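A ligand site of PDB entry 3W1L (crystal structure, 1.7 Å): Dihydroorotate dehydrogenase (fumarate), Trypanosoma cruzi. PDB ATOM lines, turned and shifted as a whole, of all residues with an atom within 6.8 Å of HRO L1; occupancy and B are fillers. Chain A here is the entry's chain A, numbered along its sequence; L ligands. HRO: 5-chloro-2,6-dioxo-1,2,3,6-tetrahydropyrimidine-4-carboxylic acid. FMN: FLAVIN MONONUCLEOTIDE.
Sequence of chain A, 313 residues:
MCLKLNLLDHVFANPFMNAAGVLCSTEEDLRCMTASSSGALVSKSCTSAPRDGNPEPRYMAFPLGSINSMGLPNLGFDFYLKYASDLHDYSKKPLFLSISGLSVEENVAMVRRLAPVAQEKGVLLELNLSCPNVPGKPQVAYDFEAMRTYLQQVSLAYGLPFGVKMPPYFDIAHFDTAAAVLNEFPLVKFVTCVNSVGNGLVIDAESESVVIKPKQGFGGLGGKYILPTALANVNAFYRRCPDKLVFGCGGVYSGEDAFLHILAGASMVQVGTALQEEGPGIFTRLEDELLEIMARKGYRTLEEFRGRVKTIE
Pro 73 touches HRO L1. CA of Cys 131 touches OAC of HRO L1, 3.5 Å away. CD of Pro 132 touches NAG of HRO L1, at 3.6 Å. Hydrophobic or aromatic side chains that line HRO L1: Met 70, Leu 72, Pro 73 and Pro 132. 12 residues have an atom within 4 Å of HRO L1: Lys 44, Asn 68, Met 70, Gly 71, Leu 72, Pro 73, Asn 128, Cys 131, Pro 132, Asn 133, Asn 195 and Ser 196.
ND2 of Asn 195 lies within hydrogen-bond range of OD1 of Asn 128 (3.4 Å). The side-chain hydroxyl of Ser 130 is in hydrogen-bond range of the side-chain amide nitrogen of Asn 195, 3.0 Å away. ND2 of Asn 133 is in hydrogen-bond range of OD1 of Asn 68 (3.0 Å). The backbone carbonyl oxygen of Asn 68 sits at hydrogen-bond distance from the backbone NH of Gly 220, at 2.9 Å. The side-chain hydroxyl (OG) of Ser 45 is in hydrogen-bond range of the side-chain amide nitrogen (ND2) of Asn 128, 3.0 Å away. OD1 of Asn 128 is in hydrogen-bond range of N of Ser 130 (2.9 Å). N of Asn 133 lies close to SG of Cys 131 (3.6 Å). O of Asn 133 lies within hydrogen-bond range of ND2 of Asn 54 (3.2 Å).
The side-chain amide oxygen (OD1) of Asn 195 lies within hydrogen-bond range of a nitrogen (NAG) of HRO L1. An oxygen (OAB) of HRO L1 is in hydrogen-bond range of the side-chain hydroxyl (OG) of Ser 196 (2.8 Å). N of Leu 72 is in hydrogen-bond range of OAD of HRO L1, 2.9 Å away. The side-chain amide oxygen (OD1) of Asn 68 is in hydrogen-bond range of a nitrogen (NAF) of HRO L1, at 2.9 Å. The side-chain amino group (NZ) of Lys 44 lies within salt-bridge range of an oxygen (OAD) of HRO L1, at 3.0 Å. An oxygen (OAC) of HRO L1 is in hydrogen-bond range of the side-chain amide nitrogen of Asn 128. The backbone NH (N) of Gly 71 lies within hydrogen-bond range of an oxygen (OAA) of HRO L1 (3.0 Å). An oxygen (OAA) of HRO L1 sits at hydrogen-bond distance from the side-chain amide nitrogen (ND2) of Asn 133 (3.1 Å). N of Met 70 is in hydrogen-bond range of OAA of HRO L1, 3.2 Å away. An oxygen (O2) of FMN L2 sits at hydrogen-bond distance from the side-chain amide nitrogen of Asn 195, 3.4 Å away. The side-chain amino group of Lys 44 lies within hydrogen-bond range of an oxygen (O4) of FMN L2. An oxygen (O2) of FMN L2 is in hydrogen-bond range of the side-chain amide nitrogen of Asn 128. N of Ser 45 sits at hydrogen-bond distance from O4 of FMN L2 (3.2 Å). The side-chain hydroxyl of Ser 45 sits at hydrogen-bond distance from a nitrogen (N3) of FMN L2 (2.9 Å). The side-chain amino group (NZ) of Lys 165 is in hydrogen-bond range of an oxygen (O2') of FMN L2, at 2.9 Å. An oxygen (O2') of FMN L2 lies within hydrogen-bond range of the backbone NH (N) of Ala 20 (3.5 Å). An oxygen (O2') of FMN L2 is in hydrogen-bond range of the backbone carbonyl oxygen of Ala 20 (2.8 Å).
A nitrogen (N3) of FMN L2 lies close to an oxygen (OAC) of HRO L1, 3.4 Å away.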
ATOM      1  N   ALA A  20     -19.383 -24.343  -6.511  1.00  0.00           N
ATOM      2  CA  ALA A  20     -20.826 -24.445  -6.713  1.00  0.00           C
ATOM      3  C   ALA A  20     -21.627 -23.951  -5.486  1.00  0.00           C
ATOM      4  O   ALA A  20     -21.214 -24.056  -4.370  1.00  0.00           O
ATOM      5  CB  ALA A  20     -21.257 -25.914  -7.036  1.00  0.00           C
ATOM      6  N   GLY A  21     -22.728 -23.288  -5.765  1.00  0.00           N
ATOM      7  CA  GLY A  21     -23.554 -22.670  -4.741  1.00  0.00           C
ATOM      8  C   GLY A  21     -23.348 -21.193  -4.486  1.00  0.00           C
ATOM      9  O   GLY A  21     -24.264 -20.533  -3.969  1.00  0.00           O
ATOM     10  N   LYS A  44     -25.342 -23.462  -9.583  1.00  0.00           N
ATOM     11  CA  LYS A  44     -25.844 -23.955  -8.298  1.00  0.00           C
ATOM     12  C   LYS A  44     -26.309 -25.381  -8.439  1.00  0.00           C
ATOM     13  O   LYS A  44     -27.063 -25.707  -9.364  1.00  0.00           O
ATOM     14  CB  LYS A  44     -27.058 -23.042  -7.908  1.00  0.00           C
ATOM     15  CG  LYS A  44     -27.892 -23.581  -6.704  1.00  0.00           C
ATOM     16  CD  LYS A  44     -27.060 -23.638  -5.400  1.00  0.00           C
ATOM     17  CE  LYS A  44     -27.707 -24.422  -4.294  1.00  0.00           C
ATOM     18  NZ  LYS A  44     -26.832 -24.400  -3.086  1.00  0.00           N
ATOM     19  N   SER A  45     -26.005 -26.253  -7.455  1.00  0.00           N
ATOM     20  CA  SER A  45     -26.508 -27.633  -7.540  1.00  0.00           C
ATOM     21  C   SER A  45     -28.027 -27.589  -7.675  1.00  0.00           C
ATOM     22  O   SER A  45     -28.678 -26.923  -6.850  1.00  0.00           O
ATOM     23  CB  SER A  45     -26.165 -28.445  -6.321  1.00  0.00           C
ATOM     24  OG  SER A  45     -24.795 -28.773  -6.335  1.00  0.00           O
ATOM     25  N   ASN A  54     -33.866 -24.275   2.905  1.00  0.00           N
ATOM     26  CA  ASN A  54     -34.128 -24.190   4.328  1.00  0.00           C
ATOM     27  C   ASN A  54     -34.480 -22.773   4.846  1.00  0.00           C
ATOM     28  O   ASN A  54     -34.292 -21.702   4.196  1.00  0.00           O
ATOM     29  CB  ASN A  54     -32.932 -24.791   5.178  1.00  0.00           C
ATOM     30  CG  ASN A  54     -32.574 -26.231   4.888  1.00  0.00           C
ATOM     31  OD1 ASN A  54     -33.434 -27.086   4.499  1.00  0.00           O
ATOM     32  ND2 ASN A  54     -31.365 -26.576   5.163  1.00  0.00           N
ATOM     33  N   ASN A  68     -23.058 -22.846   6.596  1.00  0.00           N
ATOM     34  CA  ASN A  68     -24.280 -22.749   5.775  1.00  0.00           C
ATOM     35  C   ASN A  68     -25.107 -24.003   5.887  1.00  0.00           C
ATOM     36  O   ASN A  68     -24.593 -25.128   5.968  1.00  0.00           O
ATOM     37  CB  ASN A  68     -24.024 -22.415   4.264  1.00  0.00           C
ATOM     38  CG  ASN A  68     -23.813 -23.644   3.436  1.00  0.00           C
ATOM     39  OD1 ASN A  68     -24.775 -24.375   2.991  1.00  0.00           O
ATOM     40  ND2 ASN A  68     -22.565 -24.004   3.316  1.00  0.00           N
ATOM     41  N   SER A  69     -26.422 -23.805   5.964  1.00  0.00           N
ATOM     42  CA  SER A  69     -27.344 -24.930   5.752  1.00  0.00           C
ATOM     43  C   SER A  69     -28.426 -24.459   4.743  1.00  0.00           C
ATOM     44  O   SER A  69     -29.621 -24.288   5.068  1.00  0.00           O
ATOM     45  CB  SER A  69     -27.996 -25.364   7.076  1.00  0.00           C
ATOM     46  OG  SER A  69     -28.817 -26.461   6.861  1.00  0.00           O
ATOM     47  N   MET A  70     -27.963 -24.159   3.522  1.00  0.00           N
ATOM     48  CA  MET A  70     -28.884 -23.525   2.592  1.00  0.00           C
ATOM     49  C   MET A  70     -30.124 -24.420   2.297  1.00  0.00           C
ATOM     50  O   MET A  70     -31.245 -23.909   2.174  1.00  0.00           O
ATOM     51  CB  MET A  70     -28.220 -23.208   1.291  1.00  0.00           C
ATOM     52  CG  MET A  70     -26.964 -22.411   1.333  1.00  0.00           C
ATOM     53  SD  MET A  70     -27.113 -20.776   2.132  1.00  0.00           S
ATOM     54  CE  MET A  70     -28.045 -19.913   0.929  1.00  0.00           C
ATOM     55  N   GLY A  71     -29.866 -25.708   2.140  1.00  0.00           N
ATOM     56  CA  GLY A  71     -30.920 -26.722   1.882  1.00  0.00           C
ATOM     57  C   GLY A  71     -31.227 -26.856   0.398  1.00  0.00           C
ATOM     58  O   GLY A  71     -32.385 -27.116   0.017  1.00  0.00           O
ATOM     59  N   LEU A  72     -30.243 -26.606  -0.431  1.00  0.00           N
ATOM     60  CA  LEU A  72     -30.317 -26.839  -1.905  1.00  0.00           C
ATOM     61  C   LEU A  72     -31.432 -25.966  -2.521  1.00  0.00           C
ATOM     62  O   LEU A  72     -32.196 -26.418  -3.388  1.00  0.00           O
ATOM     63  CB  LEU A  72     -30.549 -28.312  -2.135  1.00  0.00           C
ATOM     64  CG  LEU A  72     -30.380 -29.053  -3.458  1.00  0.00           C
ATOM     65  CD1 LEU A  72     -29.170 -28.516  -4.180  1.00  0.00           C
ATOM     66  CD2 LEU A  72     -30.208 -30.592  -3.152  1.00  0.00           C
ATOM     67  N   PRO A  73     -31.468 -24.724  -2.155  1.00  0.00           N
ATOM     68  CA  PRO A  73     -32.427 -23.852  -2.834  1.00  0.00           C
ATOM     69  C   PRO A  73     -31.954 -23.630  -4.288  1.00  0.00           C
ATOM     70  O   PRO A  73     -30.747 -23.385  -4.498  1.00  0.00           O
ATOM     71  CB  PRO A  73     -32.272 -22.534  -2.099  1.00  0.00           C
ATOM     72  CG  PRO A  73     -30.880 -22.546  -1.485  1.00  0.00           C
ATOM     73  CD  PRO A  73     -30.596 -23.998  -1.224  1.00  0.00           C
ATOM     74  N   SER A 100     -27.609 -32.202  -8.132  1.00  0.00           N
ATOM     75  CA  SER A 100     -27.640 -32.751  -6.832  1.00  0.00           C
ATOM     76  C   SER A 100     -29.043 -33.336  -6.570  1.00  0.00           C
ATOM     77  O   SER A 100     -29.688 -32.973  -5.637  1.00  0.00           O
ATOM     78  CB  SER A 100     -27.233 -31.687  -5.816  1.00  0.00           C
ATOM     79  OG  SER A 100     -27.040 -32.372  -4.583  1.00  0.00           O
ATOM     80  N   ASN A 128     -22.918 -33.840  -7.728  1.00  0.00           N
ATOM     81  CA  ASN A 128     -22.704 -33.547  -6.326  1.00  0.00           C
ATOM     82  C   ASN A 128     -23.064 -34.743  -5.432  1.00  0.00           C
ATOM     83  O   ASN A 128     -24.205 -35.054  -5.294  1.00  0.00           O
ATOM     84  CB  ASN A 128     -23.571 -32.351  -5.933  1.00  0.00           C
ATOM     85  CG  ASN A 128     -23.273 -31.836  -4.550  1.00  0.00           C
ATOM     86  OD1 ASN A 128     -22.500 -32.469  -3.741  1.00  0.00           O
ATOM     87  ND2 ASN A 128     -23.917 -30.767  -4.204  1.00  0.00           N
ATOM     88  N   SER A 130     -22.147 -34.866  -2.119  1.00  0.00           N
ATOM     89  CA  SER A 130     -21.663 -34.426  -0.818  1.00  0.00           C
ATOM     90  C   SER A 130     -22.442 -33.279  -0.168  1.00  0.00           C
ATOM     91  O   SER A 130     -21.905 -32.631   0.739  1.00  0.00           O
ATOM     92  CB  SER A 130     -20.177 -34.027  -0.951  1.00  0.00           C
ATOM     93  OG  SER A 130     -19.891 -33.271  -2.124  1.00  0.00           O
ATOM     94  N   CYS A 131     -23.652 -33.075  -0.550  1.00  0.00           N
ATOM     95  CA  CYS A 131     -24.501 -32.118   0.209  1.00  0.00           C
ATOM     96  C   CYS A 131     -24.698 -32.551   1.674  1.00  0.00           C
ATOM     97  O   CYS A 131     -25.220 -33.661   1.921  1.00  0.00           O
ATOM     98  CB  CYS A 131     -25.826 -31.978  -0.469  1.00  0.00           C
ATOM     99  SG  CYS A 131     -26.797 -30.753   0.491  1.00  0.00           S
ATOM    100  N   PRO A 132     -24.216 -31.725   2.657  1.00  0.00           N
ATOM    101  CA  PRO A 132     -24.386 -32.109   4.092  1.00  0.00           C
ATOM    102  C   PRO A 132     -25.577 -31.456   4.785  1.00  0.00           C
ATOM    103  O   PRO A 132     -25.654 -31.572   6.051  1.00  0.00           O
ATOM    104  CB  PRO A 132     -23.101 -31.549   4.700  1.00  0.00           C
ATOM    105  CG  PRO A 132     -22.924 -30.198   3.970  1.00  0.00           C
ATOM    106  CD  PRO A 132     -23.524 -30.429   2.586  1.00  0.00           C
ATOM    107  N   ASN A 133     -26.512 -30.831   4.047  1.00  0.00           N
ATOM    108  CA  ASN A 133     -27.542 -29.948   4.690  1.00  0.00           C
ATOM    109  C   ASN A 133     -29.014 -30.249   4.451  1.00  0.00           C
ATOM    110  O   ASN A 133     -29.851 -29.390   4.685  1.00  0.00           O
ATOM    111  CB  ASN A 133     -27.322 -28.495   4.250  1.00  0.00           C
ATOM    112  CG  ASN A 133     -26.002 -28.016   4.704  1.00  0.00           C
ATOM    113  OD1 ASN A 133     -25.592 -28.338   5.831  1.00  0.00           O
ATOM    114  ND2 ASN A 133     -25.339 -27.227   3.883  1.00  0.00           N
ATOM    115  N   VAL A 134     -29.305 -31.377   3.833  1.00  0.00           N
ATOM    116  CA  VAL A 134     -30.758 -31.724   3.574  1.00  0.00           C
ATOM    117  C   VAL A 134     -31.161 -32.765   4.648  1.00  0.00           C
ATOM    118  O   VAL A 134     -30.522 -33.834   4.767  1.00  0.00           O
ATOM    119  CB  VAL A 134     -30.978 -32.160   2.136  1.00  0.00           C
ATOM    120  CG1 VAL A 134     -32.433 -32.623   1.918  1.00  0.00           C
ATOM    121  CG2 VAL A 134     -30.741 -30.942   1.191  1.00  0.00           C
ATOM    122  N   LYS A 165     -18.277 -33.999  -7.156  1.00  0.00           N
ATOM    123  CA  LYS A 165     -17.967 -33.183  -5.960  1.00  0.00           C
ATOM    124  C   LYS A 165     -17.997 -34.033  -4.677  1.00  0.00           C
ATOM    125  O   LYS A 165     -19.040 -34.605  -4.319  1.00  0.00           O
ATOM    126  CB  LYS A 165     -18.994 -32.055  -5.865  1.00  0.00           C
ATOM    127  CG  LYS A 165     -18.717 -31.084  -4.735  1.00  0.00           C
ATOM    128  CD  LYS A 165     -17.547 -30.139  -5.024  1.00  0.00           C
ATOM    129  CE  LYS A 165     -17.538 -28.949  -4.070  1.00  0.00           C
ATOM    130  NZ  LYS A 165     -18.566 -27.936  -4.276  1.00  0.00           N
ATOM    131  N   ASN A 195     -16.199 -30.419  -0.865  1.00  0.00           N
ATOM    132  CA  ASN A 195     -17.421 -29.752  -0.304  1.00  0.00           C
ATOM    133  C   ASN A 195     -17.168 -29.303   1.113  1.00  0.00           C
ATOM    134  O   ASN A 195     -16.067 -29.520   1.662  1.00  0.00           O
ATOM    135  CB  ASN A 195     -18.620 -30.704  -0.490  1.00  0.00           C
ATOM    136  CG  ASN A 195     -19.940 -29.989  -0.677  1.00  0.00           C
ATOM    137  OD1 ASN A 195     -20.271 -29.007   0.034  1.00  0.00           O
ATOM    138  ND2 ASN A 195     -20.699 -30.426  -1.634  1.00  0.00           N
ATOM    139  N   SER A 196     -18.154 -28.633   1.716  1.00  0.00           N
ATOM    140  CA  SER A 196     -18.012 -28.095   3.049  1.00  0.00           C
ATOM    141  C   SER A 196     -17.768 -29.201   4.069  1.00  0.00           C
ATOM    142  O   SER A 196     -18.151 -30.391   3.898  1.00  0.00           O
ATOM    143  CB  SER A 196     -19.258 -27.151   3.340  1.00  0.00           C
ATOM    144  OG  SER A 196     -20.388 -27.946   3.332  1.00  0.00           O
ATOM    145  N   VAL A 197     -17.031 -28.857   5.105  1.00  0.00           N
ATOM    146  CA  VAL A 197     -16.792 -29.771   6.203  1.00  0.00           C
ATOM    147  C   VAL A 197     -18.138 -29.872   7.003  1.00  0.00           C
ATOM    148  O   VAL A 197     -18.596 -28.908   7.658  1.00  0.00           O
ATOM    149  CB  VAL A 197     -15.607 -29.298   7.005  1.00  0.00           C
ATOM    150  CG1 VAL A 197     -15.574 -30.028   8.327  1.00  0.00           C
ATOM    151  CG2 VAL A 197     -14.306 -29.432   6.276  1.00  0.00           C
ATOM    152  N   GLY A 219     -24.363 -26.903  10.306  1.00  0.00           N
ATOM    153  CA  GLY A 219     -24.183 -26.623   8.885  1.00  0.00           C
ATOM    154  C   GLY A 219     -22.783 -26.879   8.377  1.00  0.00           C
ATOM    155  O   GLY A 219     -21.886 -27.110   9.225  1.00  0.00           O
ATOM    156  N   GLY A 220     -22.582 -26.834   7.074  1.00  0.00           N
ATOM    157  CA  GLY A 220     -21.286 -27.082   6.551  1.00  0.00           C
ATOM    158  C   GLY A 220     -20.348 -25.897   6.701  1.00  0.00           C
ATOM    159  O   GLY A 220     -20.764 -24.754   6.563  1.00  0.00           O
ATOM    160  N   LEU A 221     -19.085 -26.188   6.985  1.00  0.00           N
ATOM    161  CA  LEU A 221     -18.073 -25.147   7.182  1.00  0.00           C
ATOM    162  C   LEU A 221     -17.223 -24.980   5.916  1.00  0.00           C
ATOM    163  O   LEU A 221     -16.860 -25.947   5.235  1.00  0.00           O
ATOM    164  CB  LEU A 221     -17.154 -25.524   8.302  1.00  0.00           C
ATOM    165  CG  LEU A 221     -17.769 -25.918   9.682  1.00  0.00           C
ATOM    166  CD1 LEU A 221     -16.746 -26.477  10.645  1.00  0.00           C
ATOM    167  CD2 LEU A 221     -18.396 -24.668  10.236  1.00  0.00           C
HETATM  168  OAA HRO L   1     -27.039 -26.425   1.414  1.00  0.00           O
HETATM  169  CAH HRO L   1     -26.612 -26.303   0.178  1.00  0.00           C
HETATM  170  OAD HRO L   1     -27.421 -26.010  -0.651  1.00  0.00           O
HETATM  171  CAI HRO L   1     -25.287 -26.747  -0.045  1.00  0.00           C
HETATM  172  CAJ HRO L   1     -25.060 -27.855  -0.919  1.00  0.00           C
HETATM  173 CL   HRO L   1     -26.259 -28.421  -2.170  1.00  0.00          CL
HETATM  174  CAL HRO L   1     -23.781 -28.446  -0.909  1.00  0.00           C
HETATM  175  OAC HRO L   1     -23.400 -29.375  -1.601  1.00  0.00           O
HETATM  176  NAG HRO L   1     -22.835 -27.951   0.009  1.00  0.00           N
HETATM  177  CAK HRO L   1     -23.100 -26.883   0.881  1.00  0.00           C
HETATM  178  OAB HRO L   1     -22.195 -26.533   1.670  1.00  0.00           O
HETATM  179  NAF HRO L   1     -24.321 -26.329   0.840  1.00  0.00           N
HETATM  180  N1  FMN L   2     -21.344 -27.132  -2.969  1.00  0.00           N
HETATM  181  C2  FMN L   2     -21.964 -27.763  -3.970  1.00  0.00           C
HETATM  182  O2  FMN L   2     -21.424 -28.751  -4.543  1.00  0.00           O
HETATM  183  N3  FMN L   2     -23.191 -27.389  -4.361  1.00  0.00           N
HETATM  184  C4  FMN L   2     -23.875 -26.359  -3.904  1.00  0.00           C
HETATM  185  O4  FMN L   2     -24.991 -25.970  -4.421  1.00  0.00           O
HETATM  186  C4A FMN L   2     -23.262 -25.628  -2.844  1.00  0.00           C
HETATM  187  N5  FMN L   2     -23.862 -24.558  -2.247  1.00  0.00           N
HETATM  188  C5A FMN L   2     -23.164 -23.787  -1.390  1.00  0.00           C
HETATM  189  C6  FMN L   2     -23.734 -22.644  -0.893  1.00  0.00           C
HETATM  190  C7  FMN L   2     -23.106 -21.818   0.035  1.00  0.00           C
HETATM  191  C7M FMN L   2     -23.710 -20.512   0.539  1.00  0.00           C
HETATM  192  C8  FMN L   2     -21.773 -22.214   0.452  1.00  0.00           C
HETATM  193  C8M FMN L   2     -20.993 -21.344   1.372  1.00  0.00           C
HETATM  194  C9  FMN L   2     -21.164 -23.371  -0.046  1.00  0.00           C
HETATM  195  C9A FMN L   2     -21.819 -24.185  -0.928  1.00  0.00           C
HETATM  196  N10 FMN L   2     -21.283 -25.350  -1.415  1.00  0.00           N
HETATM  197  C10 FMN L   2     -21.940 -26.068  -2.403  1.00  0.00           C
HETATM  198  C1' FMN L   2     -19.928 -25.793  -1.080  1.00  0.00           C
HETATM  199  C2' FMN L   2     -18.915 -24.988  -1.808  1.00  0.00           C
HETATM  200  O2' FMN L   2     -18.978 -25.330  -3.185  1.00  0.00           O
HETATM  201  C3' FMN L   2     -17.558 -25.381  -1.394  1.00  0.00           C
HETATM  202  O3' FMN L   2     -17.341 -26.781  -1.624  1.00  0.00           O
HETATM  203  C4' FMN L   2     -17.260 -25.058   0.085  1.00  0.00           C
HETATM  204  O4' FMN L   2     -17.900 -23.871   0.484  1.00  0.00           O
HETATM  205  C5' FMN L   2     -15.797 -25.020   0.473  1.00  0.00           C
HETATM  206  O5' FMN L   2     -15.067 -24.021  -0.217  1.00  0.00           O
HETATM  207  P   FMN L   2     -14.720 -22.603   0.536  1.00  0.00           P
HETATM  208  O1P FMN L   2     -13.818 -22.910   1.658  1.00  0.00           O
HETATM  209  O2P FMN L   2     -16.037 -21.989   0.933  1.00  0.00           O
HETATM  210  O3P FMN L   2     -14.062 -21.822  -0.578  1.00  0.00           O
